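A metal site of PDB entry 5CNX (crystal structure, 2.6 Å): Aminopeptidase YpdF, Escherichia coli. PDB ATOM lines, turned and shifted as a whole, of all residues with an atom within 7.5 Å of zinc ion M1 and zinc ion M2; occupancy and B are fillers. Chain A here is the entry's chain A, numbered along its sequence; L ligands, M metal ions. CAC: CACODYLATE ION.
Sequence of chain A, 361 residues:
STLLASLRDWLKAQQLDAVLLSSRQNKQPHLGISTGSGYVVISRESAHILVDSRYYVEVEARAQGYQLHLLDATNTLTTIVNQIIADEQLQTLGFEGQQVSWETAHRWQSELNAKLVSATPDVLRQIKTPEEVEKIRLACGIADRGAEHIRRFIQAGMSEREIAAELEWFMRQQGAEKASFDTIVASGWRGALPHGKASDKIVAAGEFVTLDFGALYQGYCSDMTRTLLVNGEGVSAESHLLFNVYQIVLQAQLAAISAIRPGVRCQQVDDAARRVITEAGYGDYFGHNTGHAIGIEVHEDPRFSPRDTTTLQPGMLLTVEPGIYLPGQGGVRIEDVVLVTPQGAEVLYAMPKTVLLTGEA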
ATOM      1  N   PHE A 181     -15.771  12.955 -26.066  1.00  0.00           N
ATOM      2  CA  PHE A 181     -17.211  12.966 -25.821  1.00  0.00           C
ATOM      3  C   PHE A 181     -17.946  12.433 -27.047  1.00  0.00           C
ATOM      4  O   PHE A 181     -17.352  12.319 -28.114  1.00  0.00           O
ATOM      5  CB  PHE A 181     -17.708  14.376 -25.496  1.00  0.00           C
ATOM      6  CG  PHE A 181     -17.406  15.391 -26.556  1.00  0.00           C
ATOM      7  CD1 PHE A 181     -18.312  15.626 -27.591  1.00  0.00           C
ATOM      8  CD2 PHE A 181     -16.190  16.078 -26.541  1.00  0.00           C
ATOM      9  CE1 PHE A 181     -18.050  16.544 -28.586  1.00  0.00           C
ATOM     10  CE2 PHE A 181     -15.904  17.009 -27.546  1.00  0.00           C
ATOM     11  CZ  PHE A 181     -16.851  17.245 -28.574  1.00  0.00           C
ATOM     12  N   ILE A 184     -20.867  14.662 -32.320  1.00  0.00           N
ATOM     13  CA  ILE A 184     -22.042  15.287 -32.913  1.00  0.00           C
ATOM     14  C   ILE A 184     -21.828  15.423 -34.410  1.00  0.00           C
ATOM     15  O   ILE A 184     -20.849  16.030 -34.847  1.00  0.00           O
ATOM     16  CB  ILE A 184     -22.319  16.668 -32.313  1.00  0.00           C
ATOM     17  CG1 ILE A 184     -22.831  16.534 -30.872  1.00  0.00           C
ATOM     18  CG2 ILE A 184     -23.310  17.435 -33.170  1.00  0.00           C
ATOM     19  CD1 ILE A 184     -22.795  17.839 -30.112  1.00  0.00           C
ATOM     20  N   PRO A 194     -28.204  21.619 -31.365  1.00  0.00           N
ATOM     21  CA  PRO A 194     -26.810  21.864 -30.927  1.00  0.00           C
ATOM     22  C   PRO A 194     -26.069  20.622 -30.422  1.00  0.00           C
ATOM     23  O   PRO A 194     -24.838  20.561 -30.504  1.00  0.00           O
ATOM     24  CB  PRO A 194     -26.980  22.886 -29.790  1.00  0.00           C
ATOM     25  CG  PRO A 194     -28.274  23.567 -30.085  1.00  0.00           C
ATOM     26  CD  PRO A 194     -29.166  22.504 -30.684  1.00  0.00           C
ATOM     27  N   HIS A 195     -26.818  19.628 -29.937  1.00  0.00           N
ATOM     28  CA  HIS A 195     -26.233  18.386 -29.435  1.00  0.00           C
ATOM     29  C   HIS A 195     -26.739  17.176 -30.162  1.00  0.00           C
ATOM     30  O   HIS A 195     -26.880  16.106 -29.574  1.00  0.00           O
ATOM     31  CB  HIS A 195     -26.499  18.234 -27.941  1.00  0.00           C
ATOM     32  CG  HIS A 195     -25.504  18.965 -27.100  1.00  0.00           C
ATOM     33  ND1 HIS A 195     -24.351  18.359 -26.643  1.00  0.00           N
ATOM     34  CD2 HIS A 195     -25.436  20.256 -26.691  1.00  0.00           C
ATOM     35  CE1 HIS A 195     -23.636  19.230 -25.962  1.00  0.00           C
ATOM     36  NE2 HIS A 195     -24.268  20.392 -25.982  1.00  0.00           N
ATOM     37  N   LEU A 211     -19.923  19.140 -37.449  1.00  0.00           N
ATOM     38  CA  LEU A 211     -19.208  18.093 -36.733  1.00  0.00           C
ATOM     39  C   LEU A 211     -18.601  18.654 -35.445  1.00  0.00           C
ATOM     40  O   LEU A 211     -17.687  19.467 -35.491  1.00  0.00           O
ATOM     41  CB  LEU A 211     -18.105  17.465 -37.600  1.00  0.00           C
ATOM     42  CG  LEU A 211     -18.570  16.785 -38.896  1.00  0.00           C
ATOM     43  CD1 LEU A 211     -18.320  17.681 -40.104  1.00  0.00           C
ATOM     44  CD2 LEU A 211     -17.902  15.420 -39.075  1.00  0.00           C
ATOM     45  N   ASP A 212     -19.153  18.216 -34.322  1.00  0.00           N
ATOM     46  CA  ASP A 212     -18.654  18.547 -33.005  1.00  0.00           C
ATOM     47  C   ASP A 212     -18.088  17.287 -32.360  1.00  0.00           C
ATOM     48  O   ASP A 212     -18.819  16.308 -32.154  1.00  0.00           O
ATOM     49  CB  ASP A 212     -19.769  19.138 -32.155  1.00  0.00           C
ATOM     50  CG  ASP A 212     -19.276  19.851 -30.916  1.00  0.00           C
ATOM     51  OD1 ASP A 212     -18.172  19.519 -30.409  1.00  0.00           O
ATOM     52  OD2 ASP A 212     -20.018  20.743 -30.452  1.00  0.00           O
ATOM     53  N   PHE A 213     -16.804  17.332 -32.029  1.00  0.00           N
ATOM     54  CA  PHE A 213     -16.092  16.124 -31.636  1.00  0.00           C
ATOM     55  C   PHE A 213     -14.782  16.492 -30.931  1.00  0.00           C
ATOM     56  O   PHE A 213     -14.389  17.659 -30.877  1.00  0.00           O
ATOM     57  CB  PHE A 213     -15.794  15.282 -32.866  1.00  0.00           C
ATOM     58  CG  PHE A 213     -14.868  15.946 -33.830  1.00  0.00           C
ATOM     59  CD1 PHE A 213     -15.329  16.926 -34.674  1.00  0.00           C
ATOM     60  CD2 PHE A 213     -13.512  15.644 -33.833  1.00  0.00           C
ATOM     61  CE1 PHE A 213     -14.466  17.568 -35.546  1.00  0.00           C
ATOM     62  CE2 PHE A 213     -12.655  16.281 -34.687  1.00  0.00           C
ATOM     63  CZ  PHE A 213     -13.136  17.241 -35.545  1.00  0.00           C
ATOM     64  N   GLY A 214     -14.082  15.487 -30.407  1.00  0.00           N
ATOM     65  CA  GLY A 214     -12.856  15.766 -29.697  1.00  0.00           C
ATOM     66  C   GLY A 214     -12.104  14.517 -29.347  1.00  0.00           C
ATOM     67  O   GLY A 214     -12.641  13.405 -29.425  1.00  0.00           O
ATOM     68  N   SER A 222      -9.509  17.500 -26.205  1.00  0.00           N
ATOM     69  CA  SER A 222      -9.712  18.511 -27.221  1.00  0.00           C
ATOM     70  C   SER A 222     -11.205  18.530 -27.554  1.00  0.00           C
ATOM     71  O   SER A 222     -11.934  17.609 -27.194  1.00  0.00           O
ATOM     72  CB  SER A 222      -8.871  18.244 -28.470  1.00  0.00           C
ATOM     73  OG  SER A 222      -9.153  16.976 -29.019  1.00  0.00           O
ATOM     74  N   ASP A 223     -11.636  19.582 -28.239  1.00  0.00           N
ATOM     75  CA  ASP A 223     -13.046  19.825 -28.500  1.00  0.00           C
ATOM     76  C   ASP A 223     -13.137  20.719 -29.726  1.00  0.00           C
ATOM     77  O   ASP A 223     -12.711  21.878 -29.661  1.00  0.00           O
ATOM     78  CB  ASP A 223     -13.678  20.485 -27.266  1.00  0.00           C
ATOM     79  CG  ASP A 223     -15.173  20.604 -27.353  1.00  0.00           C
ATOM     80  OD1 ASP A 223     -15.722  20.184 -28.382  1.00  0.00           O
ATOM     81  OD2 ASP A 223     -15.796  21.102 -26.393  1.00  0.00           O
ATOM     82  N   MET A 224     -13.625  20.196 -30.855  1.00  0.00           N
ATOM     83  CA  MET A 224     -13.703  21.006 -32.081  1.00  0.00           C
ATOM     84  C   MET A 224     -15.061  20.925 -32.821  1.00  0.00           C
ATOM     85  O   MET A 224     -15.681  19.859 -32.894  1.00  0.00           O
ATOM     86  CB  MET A 224     -12.583  20.606 -33.057  1.00  0.00           C
ATOM     87  CG  MET A 224     -12.416  21.598 -34.209  1.00  0.00           C
ATOM     88  SD  MET A 224     -10.902  21.437 -35.213  1.00  0.00           S
ATOM     89  CE  MET A 224     -10.899  19.676 -35.315  1.00  0.00           C
ATOM     90  N   THR A 225     -15.507  22.062 -33.362  1.00  0.00           N
ATOM     91  CA  THR A 225     -16.634  22.055 -34.281  1.00  0.00           C
ATOM     92  C   THR A 225     -16.309  22.744 -35.597  1.00  0.00           C
ATOM     93  O   THR A 225     -15.761  23.851 -35.605  1.00  0.00           O
ATOM     94  CB  THR A 225     -17.906  22.729 -33.708  1.00  0.00           C
ATOM     95  OG1 THR A 225     -18.285  22.104 -32.481  1.00  0.00           O
ATOM     96  CG2 THR A 225     -19.040  22.587 -34.663  1.00  0.00           C
ATOM     97  N   THR A 290     -20.902  30.963 -25.011  1.00  0.00           N
ATOM     98  CA  THR A 290     -19.949  31.160 -26.097  1.00  0.00           C
ATOM     99  C   THR A 290     -18.824  30.116 -26.008  1.00  0.00           C
ATOM    100  O   THR A 290     -18.262  29.697 -27.033  1.00  0.00           O
ATOM    101  CB  THR A 290     -19.369  32.597 -26.073  1.00  0.00           C
ATOM    102  OG1 THR A 290     -20.405  33.527 -26.401  1.00  0.00           O
ATOM    103  CG2 THR A 290     -18.224  32.765 -27.063  1.00  0.00           C
ATOM    104  N   GLY A 291     -18.513  29.655 -24.802  1.00  0.00           N
ATOM    105  CA  GLY A 291     -17.500  28.626 -24.673  1.00  0.00           C
ATOM    106  C   GLY A 291     -17.293  28.138 -23.246  1.00  0.00           C
ATOM    107  O   GLY A 291     -18.031  28.526 -22.321  1.00  0.00           O
ATOM    108  N   HIS A 292     -16.318  27.254 -23.072  1.00  0.00           N
ATOM    109  CA  HIS A 292     -16.036  26.684 -21.767  1.00  0.00           C
ATOM    110  C   HIS A 292     -14.560  26.359 -21.654  1.00  0.00           C
ATOM    111  O   HIS A 292     -13.880  26.111 -22.655  1.00  0.00           O
ATOM    112  CB  HIS A 292     -16.869  25.425 -21.547  1.00  0.00           C
ATOM    113  CG  HIS A 292     -16.717  24.421 -22.640  1.00  0.00           C
ATOM    114  ND1 HIS A 292     -15.674  23.522 -22.679  1.00  0.00           N
ATOM    115  CD2 HIS A 292     -17.472  24.174 -23.723  1.00  0.00           C
ATOM    116  CE1 HIS A 292     -15.793  22.763 -23.760  1.00  0.00           C
ATOM    117  NE2 HIS A 292     -16.879  23.135 -24.403  1.00  0.00           N
ATOM    118  N   ALA A 293     -14.056  26.345 -20.429  1.00  0.00           N
ATOM    119  CA  ALA A 293     -12.679  25.911 -20.222  1.00  0.00           C
ATOM    120  C   ALA A 293     -12.593  24.412 -20.519  1.00  0.00           C
ATOM    121  O   ALA A 293     -13.613  23.697 -20.514  1.00  0.00           O
ATOM    122  CB  ALA A 293     -12.210  26.216 -18.825  1.00  0.00           C
ATOM    123  N   ILE A 294     -11.376  23.926 -20.770  1.00  0.00           N
ATOM    124  CA  ILE A 294     -11.183  22.520 -21.097  1.00  0.00           C
ATOM    125  C   ILE A 294      -9.837  22.079 -20.546  1.00  0.00           C
ATOM    126  O   ILE A 294      -8.935  22.893 -20.406  1.00  0.00           O
ATOM    127  CB  ILE A 294     -11.264  22.260 -22.623  1.00  0.00           C
ATOM    128  CG1 ILE A 294     -11.123  20.770 -22.941  1.00  0.00           C
ATOM    129  CG2 ILE A 294     -10.206  23.075 -23.364  1.00  0.00           C
ATOM    130  CD1 ILE A 294     -11.523  20.411 -24.353  1.00  0.00           C
ATOM    131  N   VAL A 298     -13.665  17.825 -20.467  1.00  0.00           N
ATOM    132  CA  VAL A 298     -14.149  18.586 -21.617  1.00  0.00           C
ATOM    133  C   VAL A 298     -14.769  19.916 -21.174  1.00  0.00           C
ATOM    134  O   VAL A 298     -14.548  20.935 -21.827  1.00  0.00           O
ATOM    135  CB  VAL A 298     -15.137  17.744 -22.447  1.00  0.00           C
ATOM    136  CG1 VAL A 298     -16.047  18.600 -23.323  1.00  0.00           C
ATOM    137  CG2 VAL A 298     -14.383  16.692 -23.262  1.00  0.00           C
ATOM    138  N   HIS A 299     -15.544  19.902 -20.095  1.00  0.00           N
ATOM    139  CA  HIS A 299     -16.118  21.143 -19.575  1.00  0.00           C
ATOM    140  C   HIS A 299     -15.534  21.514 -18.224  1.00  0.00           C
ATOM    141  O   HIS A 299     -15.748  20.825 -17.236  1.00  0.00           O
ATOM    142  CB  HIS A 299     -17.632  21.010 -19.462  1.00  0.00           C
ATOM    143  CG  HIS A 299     -18.289  20.684 -20.757  1.00  0.00           C
ATOM    144  ND1 HIS A 299     -18.717  19.412 -21.072  1.00  0.00           N
ATOM    145  CD2 HIS A 299     -18.576  21.456 -21.829  1.00  0.00           C
ATOM    146  CE1 HIS A 299     -19.249  19.422 -22.287  1.00  0.00           C
ATOM    147  NE2 HIS A 299     -19.175  20.646 -22.760  1.00  0.00           N
ATOM    148  N   THR A 319     -12.859  27.109 -24.939  1.00  0.00           N
ATOM    149  CA  THR A 319     -13.385  26.995 -26.293  1.00  0.00           C
ATOM    150  C   THR A 319     -14.111  28.272 -26.669  1.00  0.00           C
ATOM    151  O   THR A 319     -14.580  29.006 -25.785  1.00  0.00           O
ATOM    152  CB  THR A 319     -14.344  25.793 -26.460  1.00  0.00           C
ATOM    153  OG1 THR A 319     -15.514  25.962 -25.636  1.00  0.00           O
ATOM    154  CG2 THR A 319     -13.637  24.475 -26.105  1.00  0.00           C
ATOM    155  N   VAL A 320     -14.153  28.568 -27.974  1.00  0.00           N
ATOM    156  CA  VAL A 320     -15.013  29.630 -28.516  1.00  0.00           C
ATOM    157  C   VAL A 320     -15.919  29.021 -29.585  1.00  0.00           C
ATOM    158  O   VAL A 320     -15.439  28.671 -30.673  1.00  0.00           O
ATOM    159  CB  VAL A 320     -14.228  30.785 -29.135  1.00  0.00           C
ATOM    160  CG1 VAL A 320     -15.192  31.821 -29.714  1.00  0.00           C
ATOM    161  CG2 VAL A 320     -13.266  31.419 -28.126  1.00  0.00           C
ATOM    162  N   GLU A 321     -17.205  28.862 -29.261  1.00  0.00           N
ATOM    163  CA  GLU A 321     -18.125  28.102 -30.106  1.00  0.00           C
ATOM    164  C   GLU A 321     -19.539  28.670 -30.193  1.00  0.00           C
ATOM    165  O   GLU A 321     -20.509  28.027 -29.787  1.00  0.00           O
ATOM    166  CB  GLU A 321     -18.192  26.671 -29.588  1.00  0.00           C
ATOM    167  CG  GLU A 321     -18.276  26.588 -28.081  1.00  0.00           C
ATOM    168  CD  GLU A 321     -18.477  25.182 -27.582  1.00  0.00           C
ATOM    169  OE1 GLU A 321     -19.160  24.386 -28.271  1.00  0.00           O
ATOM    170  OE2 GLU A 321     -17.941  24.866 -26.512  1.00  0.00           O
ATOM    171  N   ARG A 333     -22.413  26.052 -36.329  1.00  0.00           N
ATOM    172  CA  ARG A 333     -21.528  26.301 -35.196  1.00  0.00           C
ATOM    173  C   ARG A 333     -20.083  26.138 -35.624  1.00  0.00           C
ATOM    174  O   ARG A 333     -19.770  25.269 -36.443  1.00  0.00           O
ATOM    175  CB  ARG A 333     -21.835  25.359 -34.025  1.00  0.00           C
ATOM    176  CG  ARG A 333     -20.886  25.553 -32.831  1.00  0.00           C
ATOM    177  CD  ARG A 333     -21.334  24.810 -31.579  1.00  0.00           C
ATOM    178  NE  ARG A 333     -21.340  23.366 -31.792  1.00  0.00           N
ATOM    179  CZ  ARG A 333     -22.444  22.669 -32.059  1.00  0.00           C
ATOM    180  NH1 ARG A 333     -23.614  23.291 -32.125  1.00  0.00           N
ATOM    181  NH2 ARG A 333     -22.387  21.355 -32.249  1.00  0.00           N
ATOM    182  N   GLU A 335     -16.257  25.960 -33.716  1.00  0.00           N
ATOM    183  CA  GLU A 335     -15.593  25.881 -32.418  1.00  0.00           C
ATOM    184  C   GLU A 335     -14.076  25.726 -32.480  1.00  0.00           C
ATOM    185  O   GLU A 335     -13.558  24.842 -33.171  1.00  0.00           O
ATOM    186  CB  GLU A 335     -16.202  24.733 -31.607  1.00  0.00           C
ATOM    187  CG  GLU A 335     -15.512  24.426 -30.285  1.00  0.00           C
ATOM    188  CD  GLU A 335     -16.325  23.411 -29.474  1.00  0.00           C
ATOM    189  OE1 GLU A 335     -17.048  22.596 -30.095  1.00  0.00           O
ATOM    190  OE2 GLU A 335     -16.206  23.423 -28.228  1.00  0.00           O
ATOM    191  N   ASP A 336     -13.386  26.588 -31.744  1.00  0.00           N
ATOM    192  CA  ASP A 336     -11.944  26.486 -31.570  1.00  0.00           C
ATOM    193  C   ASP A 336     -11.610  26.293 -30.098  1.00  0.00           C
ATOM    194  O   ASP A 336     -12.355  26.752 -29.220  1.00  0.00           O
ATOM    195  CB  ASP A 336     -11.234  27.743 -32.060  1.00  0.00           C
ATOM    196  CG  ASP A 336     -11.140  27.809 -33.570  1.00  0.00           C
ATOM    197  OD1 ASP A 336     -10.993  26.739 -34.205  1.00  0.00           O
ATOM    198  OD2 ASP A 336     -11.176  28.940 -34.103  1.00  0.00           O
ATOM    199  N   VAL A 337     -10.501  25.610 -29.818  1.00  0.00           N
ATOM    200  CA  VAL A 337      -9.905  25.673 -28.487  1.00  0.00           C
ATOM    201  C   VAL A 337      -8.868  26.796 -28.518  1.00  0.00           C
ATOM    202  O   VAL A 337      -8.026  26.853 -29.413  1.00  0.00           O
ATOM    203  CB  VAL A 337      -9.238  24.358 -28.057  1.00  0.00           C
ATOM    204  CG1 VAL A 337      -8.281  24.595 -26.890  1.00  0.00           C
ATOM    205  CG2 VAL A 337     -10.291  23.326 -27.677  1.00  0.00           C
HETATM  206 AS   CAC L   1     -19.406  20.544 -26.450  1.00  0.00          AS
HETATM  207  O1  CAC L   1     -18.387  21.514 -27.479  1.00  0.00           O
HETATM  208  O2  CAC L   1     -18.494  19.330 -25.603  1.00  0.00           O
HETATM  209  C1  CAC L   1     -20.343  21.760 -25.213  1.00  0.00           C
HETATM  210  C2  CAC L   1     -20.733  19.599 -27.543  1.00  0.00           C
HETATM  211 ZN    ZN M   1     -17.203  22.869 -26.527  1.00  0.00          ZN
HETATM  212 ZN    ZN M   2     -17.542  21.033 -29.133  1.00  0.00          ZN
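Zinc ion M2 is bound by OE1 of Glu 335 (1.9 Å), O1 of the ligand (1.9 Å), OD1 of Asp 212 (2.1 Å) and OD1 of Asp 223 (2.1 Å).
Slightly farther from zinc ion M2 lies OD2 of Asp 212 (2.8 Å).
Merely in contact with zinc ion M1: Thr 319 (3.6 Å).
Of the 26 residues printed, 5 come within 4 Å of zinc ion M1.
The nearest printed residue that does not touch zinc ion M1 is His 299 (4.8 Å).
Zinc ion M1 is bound by an oxygen (O1) of the ligand, the side-chain carboxylate of Glu 335, the side-chain carboxylate of Glu 321, a ring nitrogen (NE2) of His 292 and the side-chain carboxylate of Asp 223.
Zinc ion M1 has five donor atoms within binding distance.
Residues that only touch zinc ion M2: Thr 225 and Phe 181.
Six residues have an atom within 4 Å of zinc ion M2: Phe 181, Asp 212, Asp 223, Thr 225, Glu 321 and Glu 335.
Along chain A the residues within 4 Å of zinc ion M2 span positions 181 to 335.
The nearest printed residue that does not touch zinc ion M2 is Met 224 (4.4 Å).
OG1 of Thr 225 is in hydrogen-bond range of NE of Arg 333 (3.4 Å).
The side-chain hydroxyl (OG1) of Thr 319 sits close to the side-chain carboxylate (OE2) of Glu 321, 2.8 Å away.
The backbone NH (N) of Ile 184 is in hydrogen-bond range of the backbone carbonyl oxygen (O) of Asp 212 (2.6 Å).
ND1 of His 292 sits close to O of Val 298 (2.9 Å).
The backbone NH (N) of Glu 321 sits at hydrogen-bond distance from the backbone carbonyl oxygen (O) of Thr 290 (2.6 Å).
The backbone NH of Glu 335 is in hydrogen-bond range of the backbone carbonyl oxygen of Thr 225, 2.9 Å away.
The guanidinium group (NH2) of Arg 333 is in salt-bridge range of the side-chain carboxylate (OD2) of Asp 212, at 3.0 Å.
O of His 292 lies within hydrogen-bond range of N of Thr 319.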
